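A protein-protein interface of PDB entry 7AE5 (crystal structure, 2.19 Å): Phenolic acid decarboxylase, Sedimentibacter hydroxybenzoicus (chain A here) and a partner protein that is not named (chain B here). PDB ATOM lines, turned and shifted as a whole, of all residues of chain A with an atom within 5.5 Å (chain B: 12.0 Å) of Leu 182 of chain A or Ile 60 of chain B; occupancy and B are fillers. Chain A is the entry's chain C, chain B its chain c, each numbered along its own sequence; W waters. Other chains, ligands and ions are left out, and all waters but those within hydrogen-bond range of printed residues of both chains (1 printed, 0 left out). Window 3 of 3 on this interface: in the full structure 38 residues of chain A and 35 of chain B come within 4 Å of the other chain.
CD2 of Leu 182 of chain A touches CG2 of Ile 60 of chain B, 3.8 Å away. CG1 of Val 59 of chain B touches CG of Arg 270 of chain A, 3.6 Å away. Arg 270 of chain A touches Ile 60 of chain B. Arg 270 of chain A touches Pro 62 of chain B. CG of Arg 270 of chain A touches CD1 of Ile 63 of chain B (3.6 Å). Met 57 of chain B touches Arg 287 of chain A. O of Gly 58 of chain B touches CB of Arg 287 of chain A (3.6 Å). SD of Met 57 of chain B touches N of Leu 288 of chain A (3.9 Å). Val 59 of chain B touches Leu 288 of chain A (CA to O, 3.6 Å). Pro 61 of chain B touches Cys 290 of chain A.
The backbone carbonyl oxygen of Ile 60 of chain B lies close to the side-chain amide oxygen of Gln 289 of chain A, at 3.4 Å. The backbone carbonyl oxygen (O) of Pro 61 of chain B sits at hydrogen-bond distance from the guanidinium group (NE) of Arg 270 of chain A, at 2.9 Å. The backbone carbonyl oxygen (O) of Leu 288 of chain A is in hydrogen-bond range of the backbone NH (N) of Ile 60 of chain B. O of Gly 58 of chain B sits at hydrogen-bond distance from N of Leu 288 of chain A (3.0 Å).
Water W1 lies within hydrogen-bond range of O of Ile 60 of chain B (2.8 Å), N of Cys 290 of chain A (2.9 Å), N of Ala 181 of chain A (3.0 Å) and OE1 of Gln 289 of chain A (3.0 Å).
Of the 11 printed residues of chain A, 6 touch a printed residue of chain B. Hydrophobic or aromatic side chains of chain A that line the printed part of chain B: Leu 182 and Leu 288. Along chain A the printed residues that touch a printed residue of chain B span positions 182 to 290. Printed residues of chain B that touch a printed residue of chain A: Met 57, Gly 58, Val 59, Ile 60, Pro 61, Pro 62 and Ile 63. Among the printed residues, 15 pairs touch across the chains. Among the printed residues, no Asp or Glu carboxylate lies within 4 Å of a Lys or Arg side-chain nitrogen of the other chain.
Leu 182 of chain A touches just one residue of chain B: Ile 60 (3.8 Å). Ile 60 of chain B touches just these residues of chain A: Leu 182, Arg 270, Arg 287, Leu 288 and Gln 289. No residue of chain B comes within 4 Å of Ala 181 of chain A. Ala 183 of chain A touches none of the printed residues of chain B. No residue of chain B comes within 4 Å of Met 184 of chain A. Of the printed residues of chain B, Leu 288 of chain A touches Met 57 (3.9 Å), Gly 58 (3.0 Å), Val 59 (3.6 Å) and Ile 60 (2.9 Å). Gln 289 of chain A touches one residue of chain B. Of the printed residues of chain B, Cys 290 of chain A touches Pro 61. Printed residues of chain A within 4 Å of Pro 61 of chain B: Arg 270 and Cys 290. Of the printed residues of chain A, Met 57 of chain B touches Arg 287 and Leu 288. The nearest residue of chain B that does not touch Leu 182 of chain A is Pro 61 of chain B (4.3 Å). The nearest residue of chain A that does not touch Ile 60 of chain B is Cys 290 of chain A (4.1 Å). The nearest printed residue of chain A that does not touch Pro 62 of chain B is Leu 182 of chain A (5.6 Å).
The side-chain sulfur (SG) of Cys 290 of chain A is in hydrogen-bond range of the guanidinium group (NH1) of Arg 270 of chain A.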
ATOM      1  N   GLN A 180      14.225 -21.944   9.112  1.00  0.00           N
ATOM      2  CA  GLN A 180      14.973 -22.915   8.316  1.00  0.00           C
ATOM      3  C   GLN A 180      14.398 -22.893   6.906  1.00  0.00           C
ATOM      4  O   GLN A 180      13.483 -23.646   6.572  1.00  0.00           O
ATOM      5  CB  GLN A 180      14.892 -24.299   8.945  1.00  0.00           C
ATOM      6  CG  GLN A 180      15.666 -24.434  10.242  1.00  0.00           C
ATOM      7  CD  GLN A 180      15.528 -25.811  10.852  1.00  0.00           C
ATOM      8  OE1 GLN A 180      14.420 -26.266  11.142  1.00  0.00           O
ATOM      9  NE2 GLN A 180      16.654 -26.492  11.039  1.00  0.00           N
ATOM     10  N   ALA A 181      14.952 -22.016   6.065  1.00  0.00           N
ATOM     11  CA  ALA A 181      14.373 -21.776   4.745  1.00  0.00           C
ATOM     12  C   ALA A 181      14.470 -23.007   3.851  1.00  0.00           C
ATOM     13  O   ALA A 181      13.561 -23.271   3.054  1.00  0.00           O
ATOM     14  CB  ALA A 181      15.053 -20.577   4.089  1.00  0.00           C
ATOM     15  N   LEU A 182      15.563 -23.768   3.957  1.00  0.00           N
ATOM     16  CA  LEU A 182      15.692 -24.991   3.170  1.00  0.00           C
ATOM     17  C   LEU A 182      14.729 -26.072   3.648  1.00  0.00           C
ATOM     18  O   LEU A 182      14.342 -26.938   2.855  1.00  0.00           O
ATOM     19  CB  LEU A 182      17.141 -25.495   3.215  1.00  0.00           C
ATOM     20  CG  LEU A 182      17.606 -26.734   2.434  1.00  0.00           C
ATOM     21  CD1 LEU A 182      16.852 -26.928   1.123  1.00  0.00           C
ATOM     22  CD2 LEU A 182      19.100 -26.645   2.162  1.00  0.00           C
ATOM     23  N   ALA A 183      14.316 -26.037   4.918  1.00  0.00           N
ATOM     24  CA  ALA A 183      13.274 -26.949   5.372  1.00  0.00           C
ATOM     25  C   ALA A 183      11.934 -26.667   4.703  1.00  0.00           C
ATOM     26  O   ALA A 183      11.073 -27.553   4.669  1.00  0.00           O
ATOM     27  CB  ALA A 183      13.127 -26.877   6.894  1.00  0.00           C
ATOM     28  N   MET A 184      11.740 -25.459   4.175  1.00  0.00           N
ATOM     29  CA  MET A 184      10.564 -25.125   3.379  1.00  0.00           C
ATOM     30  C   MET A 184      10.885 -25.371   1.910  1.00  0.00           C
ATOM     31  O   MET A 184      11.751 -24.699   1.339  1.00  0.00           O
ATOM     32  CB  MET A 184      10.148 -23.673   3.605  1.00  0.00           C
ATOM     33  CG  MET A 184      10.391 -23.168   5.017  1.00  0.00           C
ATOM     34  SD  MET A 184      10.646 -21.383   5.082  1.00  0.00           S
ATOM     35  CE  MET A 184       8.955 -20.803   4.969  1.00  0.00           C
ATOM     36  N   HIS A 185      10.183 -26.322   1.296  1.00  0.00           N
ATOM     37  CA  HIS A 185      10.592 -26.827  -0.010  1.00  0.00           C
ATOM     38  C   HIS A 185       9.979 -26.060  -1.176  1.00  0.00           C
ATOM     39  O   HIS A 185      10.639 -25.882  -2.206  1.00  0.00           O
ATOM     40  CB  HIS A 185      10.250 -28.314  -0.119  1.00  0.00           C
ATOM     41  CG  HIS A 185      11.190 -29.199   0.638  1.00  0.00           C
ATOM     42  ND1 HIS A 185      10.757 -30.210   1.468  1.00  0.00           N
ATOM     43  CD2 HIS A 185      12.542 -29.215   0.699  1.00  0.00           C
ATOM     44  CE1 HIS A 185      11.803 -30.816   2.003  1.00  0.00           C
ATOM     45  NE2 HIS A 185      12.898 -30.230   1.552  1.00  0.00           N
ATOM     46  N   ARG A 270      22.314 -14.213   6.616  1.00  0.00           N
ATOM     47  CA  ARG A 270      22.463 -15.475   7.325  1.00  0.00           C
ATOM     48  C   ARG A 270      23.069 -15.195   8.690  1.00  0.00           C
ATOM     49  O   ARG A 270      24.131 -14.571   8.784  1.00  0.00           O
ATOM     50  CB  ARG A 270      23.342 -16.456   6.543  1.00  0.00           C
ATOM     51  CG  ARG A 270      22.814 -16.787   5.161  1.00  0.00           C
ATOM     52  CD  ARG A 270      21.574 -17.664   5.224  1.00  0.00           C
ATOM     53  NE  ARG A 270      21.232 -18.193   3.910  1.00  0.00           N
ATOM     54  CZ  ARG A 270      20.609 -17.506   2.964  1.00  0.00           C
ATOM     55  NH1 ARG A 270      20.217 -16.257   3.160  1.00  0.00           N
ATOM     56  NH2 ARG A 270      20.370 -18.086   1.790  1.00  0.00           N
ATOM     57  N   ARG A 287      23.545 -23.347  12.974  1.00  0.00           N
ATOM     58  CA  ARG A 287      23.919 -23.079  11.595  1.00  0.00           C
ATOM     59  C   ARG A 287      23.614 -21.625  11.267  1.00  0.00           C
ATOM     60  O   ARG A 287      22.863 -20.951  11.977  1.00  0.00           O
ATOM     61  CB  ARG A 287      23.183 -24.003  10.613  1.00  0.00           C
ATOM     62  CG  ARG A 287      23.415 -25.489  10.847  1.00  0.00           C
ATOM     63  CD  ARG A 287      24.657 -25.984  10.119  1.00  0.00           C
ATOM     64  NE  ARG A 287      24.777 -27.437  10.174  1.00  0.00           N
ATOM     65  CZ  ARG A 287      25.270 -28.110  11.204  1.00  0.00           C
ATOM     66  NH1 ARG A 287      25.709 -27.491  12.288  1.00  0.00           N
ATOM     67  NH2 ARG A 287      25.326 -29.438  11.146  1.00  0.00           N
ATOM     68  N   LEU A 288      24.210 -21.147  10.179  1.00  0.00           N
ATOM     69  CA  LEU A 288      23.912 -19.813   9.668  1.00  0.00           C
ATOM     70  C   LEU A 288      22.668 -19.910   8.792  1.00  0.00           C
ATOM     71  O   LEU A 288      22.732 -20.414   7.666  1.00  0.00           O
ATOM     72  CB  LEU A 288      25.102 -19.257   8.893  1.00  0.00           C
ATOM     73  CG  LEU A 288      26.257 -18.714   9.740  1.00  0.00           C
ATOM     74  CD1 LEU A 288      27.418 -18.282   8.863  1.00  0.00           C
ATOM     75  CD2 LEU A 288      25.795 -17.562  10.613  1.00  0.00           C
ATOM     76  N   GLN A 289      21.537 -19.439   9.307  1.00  0.00           N
ATOM     77  CA  GLN A 289      20.247 -19.642   8.667  1.00  0.00           C
ATOM     78  C   GLN A 289      19.593 -18.306   8.331  1.00  0.00           C
ATOM     79  O   GLN A 289      20.052 -17.235   8.737  1.00  0.00           O
ATOM     80  CB  GLN A 289      19.326 -20.483   9.560  1.00  0.00           C
ATOM     81  CG  GLN A 289      19.964 -21.778  10.043  1.00  0.00           C
ATOM     82  CD  GLN A 289      19.354 -23.008   9.399  1.00  0.00           C
ATOM     83  OE1 GLN A 289      18.921 -22.967   8.248  1.00  0.00           O
ATOM     84  NE2 GLN A 289      19.330 -24.113  10.136  1.00  0.00           N
ATOM     85  N   CYS A 290      18.501 -18.391   7.578  1.00  0.00           N
ATOM     86  CA  CYS A 290      17.797 -17.204   7.120  1.00  0.00           C
ATOM     87  C   CYS A 290      17.083 -16.512   8.272  1.00  0.00           C
ATOM     88  O   CYS A 290      16.640 -17.147   9.233  1.00  0.00           O
ATOM     89  CB  CYS A 290      16.783 -17.571   6.040  1.00  0.00           C
ATOM     90  SG  CYS A 290      17.522 -17.913   4.440  1.00  0.00           S
ATOM     91  N   LYS B  53      34.677 -21.231  14.984  1.00  0.00           N
ATOM     92  CA  LYS B  53      33.480 -22.038  14.775  1.00  0.00           C
ATOM     93  C   LYS B  53      32.393 -21.247  14.060  1.00  0.00           C
ATOM     94  O   LYS B  53      31.631 -21.819  13.273  1.00  0.00           O
ATOM     95  CB  LYS B  53      32.948 -22.578  16.105  1.00  0.00           C
ATOM     96  CG  LYS B  53      33.708 -23.785  16.636  1.00  0.00           C
ATOM     97  CD  LYS B  53      34.516 -23.451  17.877  1.00  0.00           C
ATOM     98  CE  LYS B  53      35.609 -24.480  18.128  1.00  0.00           C
ATOM     99  NZ  LYS B  53      36.730 -24.353  17.152  1.00  0.00           N
ATOM    100  N   ILE B  54      32.312 -19.938  14.311  1.00  0.00           N
ATOM    101  CA  ILE B  54      31.321 -19.109  13.631  1.00  0.00           C
ATOM    102  C   ILE B  54      31.694 -18.917  12.167  1.00  0.00           C
ATOM    103  O   ILE B  54      30.842 -19.018  11.275  1.00  0.00           O
ATOM    104  CB  ILE B  54      31.164 -17.762  14.360  1.00  0.00           C
ATOM    105  CG1 ILE B  54      30.217 -17.913  15.551  1.00  0.00           C
ATOM    106  CG2 ILE B  54      30.663 -16.686  13.410  1.00  0.00           C
ATOM    107  CD1 ILE B  54      30.303 -16.777  16.543  1.00  0.00           C
ATOM    108  N   ALA B  55      32.973 -18.646  11.892  1.00  0.00           N
ATOM    109  CA  ALA B  55      33.416 -18.494  10.510  1.00  0.00           C
ATOM    110  C   ALA B  55      33.289 -19.797   9.728  1.00  0.00           C
ATOM    111  O   ALA B  55      32.991 -19.769   8.529  1.00  0.00           O
ATOM    112  CB  ALA B  55      34.861 -17.993  10.474  1.00  0.00           C
ATOM    113  N   ASN B  56      33.514 -20.938  10.379  1.00  0.00           N
ATOM    114  CA  ASN B  56      33.417 -22.243   9.740  1.00  0.00           C
ATOM    115  C   ASN B  56      32.006 -22.820   9.782  1.00  0.00           C
ATOM    116  O   ASN B  56      31.809 -23.976   9.394  1.00  0.00           O
ATOM    117  CB  ASN B  56      34.392 -23.226  10.397  1.00  0.00           C
ATOM    118  CG  ASN B  56      35.844 -22.874  10.135  1.00  0.00           C
ATOM    119  OD1 ASN B  56      36.152 -21.783   9.659  1.00  0.00           O
ATOM    120  ND2 ASN B  56      36.746 -23.796  10.458  1.00  0.00           N
ATOM    121  N   MET B  57      31.027 -22.045  10.240  1.00  0.00           N
ATOM    122  CA  MET B  57      29.668 -22.553  10.374  1.00  0.00           C
ATOM    123  C   MET B  57      29.013 -22.708   9.007  1.00  0.00           C
ATOM    124  O   MET B  57      29.181 -21.868   8.118  1.00  0.00           O
ATOM    125  CB  MET B  57      28.842 -21.617  11.254  1.00  0.00           C
ATOM    126  CG  MET B  57      27.602 -22.257  11.847  1.00  0.00           C
ATOM    127  SD  MET B  57      26.789 -21.186  13.047  1.00  0.00           S
ATOM    128  CE  MET B  57      27.797 -21.467  14.503  1.00  0.00           C
ATOM    129  N   GLY B  58      28.257 -23.792   8.846  1.00  0.00           N
ATOM    130  CA  GLY B  58      27.617 -24.067   7.570  1.00  0.00           C
ATOM    131  C   GLY B  58      26.481 -23.095   7.299  1.00  0.00           C
ATOM    132  O   GLY B  58      25.616 -22.871   8.154  1.00  0.00           O
ATOM    133  N   VAL B  59      26.477 -22.519   6.101  1.00  0.00           N
ATOM    134  CA  VAL B  59      25.477 -21.540   5.688  1.00  0.00           C
ATOM    135  C   VAL B  59      24.375 -22.274   4.935  1.00  0.00           C
ATOM    136  O   VAL B  59      24.625 -22.876   3.884  1.00  0.00           O
ATOM    137  CB  VAL B  59      26.102 -20.440   4.818  1.00  0.00           C
ATOM    138  CG1 VAL B  59      25.040 -19.458   4.362  1.00  0.00           C
ATOM    139  CG2 VAL B  59      27.208 -19.730   5.577  1.00  0.00           C
ATOM    140  N   ILE B  60      23.152 -22.216   5.465  1.00  0.00           N
ATOM    141  CA  ILE B  60      22.031 -22.983   4.944  1.00  0.00           C
ATOM    142  C   ILE B  60      20.864 -22.042   4.672  1.00  0.00           C
ATOM    143  O   ILE B  60      20.368 -21.393   5.599  1.00  0.00           O
ATOM    144  CB  ILE B  60      21.591 -24.096   5.910  1.00  0.00           C
ATOM    145  CG1 ILE B  60      22.801 -24.906   6.390  1.00  0.00           C
ATOM    146  CG2 ILE B  60      20.549 -24.987   5.248  1.00  0.00           C
ATOM    147  CD1 ILE B  60      22.465 -26.306   6.866  1.00  0.00           C
ATOM    148  N   PRO B  61      20.393 -21.910   3.420  1.00  0.00           N
ATOM    149  CA  PRO B  61      21.004 -22.427   2.191  1.00  0.00           C
ATOM    150  C   PRO B  61      22.092 -21.466   1.712  1.00  0.00           C
ATOM    151  O   PRO B  61      22.230 -20.396   2.305  1.00  0.00           O
ATOM    152  CB  PRO B  61      19.825 -22.477   1.219  1.00  0.00           C
ATOM    153  CG  PRO B  61      18.970 -21.348   1.652  1.00  0.00           C
ATOM    154  CD  PRO B  61      19.069 -21.319   3.154  1.00  0.00           C
ATOM    155  N   PRO B  62      22.859 -21.833   0.684  1.00  0.00           N
ATOM    156  CA  PRO B  62      23.884 -20.908   0.183  1.00  0.00           C
ATOM    157  C   PRO B  62      23.262 -19.656  -0.415  1.00  0.00           C
ATOM    158  O   PRO B  62      22.197 -19.701  -1.038  1.00  0.00           O
ATOM    159  CB  PRO B  62      24.622 -21.731  -0.882  1.00  0.00           C
ATOM    160  CG  PRO B  62      24.300 -23.152  -0.568  1.00  0.00           C
ATOM    161  CD  PRO B  62      22.920 -23.137   0.003  1.00  0.00           C
ATOM    162  N   ILE B  63      23.935 -18.529  -0.210  1.00  0.00           N
ATOM    163  CA  ILE B  63      23.509 -17.256  -0.784  1.00  0.00           C
ATOM    164  C   ILE B  63      23.961 -17.206  -2.239  1.00  0.00           C
ATOM    165  O   ILE B  63      25.170 -17.226  -2.511  1.00  0.00           O
ATOM    166  CB  ILE B  63      24.072 -16.062   0.004  1.00  0.00           C
ATOM    167  CG1 ILE B  63      23.612 -16.108   1.461  1.00  0.00           C
ATOM    168  CG2 ILE B  63      23.651 -14.751  -0.645  1.00  0.00           C
ATOM    169  CD1 ILE B  63      24.310 -15.098   2.344  1.00  0.00           C
ATOM    170  N   PRO B  64      23.042 -17.138  -3.196  1.00  0.00           N
ATOM    171  CA  PRO B  64      23.441 -17.036  -4.601  1.00  0.00           C
ATOM    172  C   PRO B  64      24.091 -15.693  -4.876  1.00  0.00           C
ATOM    173  O   PRO B  64      23.914 -14.740  -4.102  1.00  0.00           O
ATOM    174  CB  PRO B  64      22.111 -17.178  -5.356  1.00  0.00           C
ATOM    175  CG  PRO B  64      21.089 -16.678  -4.389  1.00  0.00           C
ATOM    176  CD  PRO B  64      21.578 -17.103  -3.031  1.00  0.00           C
HETATM  177  O   HOH W   1      17.722 -20.949   6.368  1.00  0.00           O
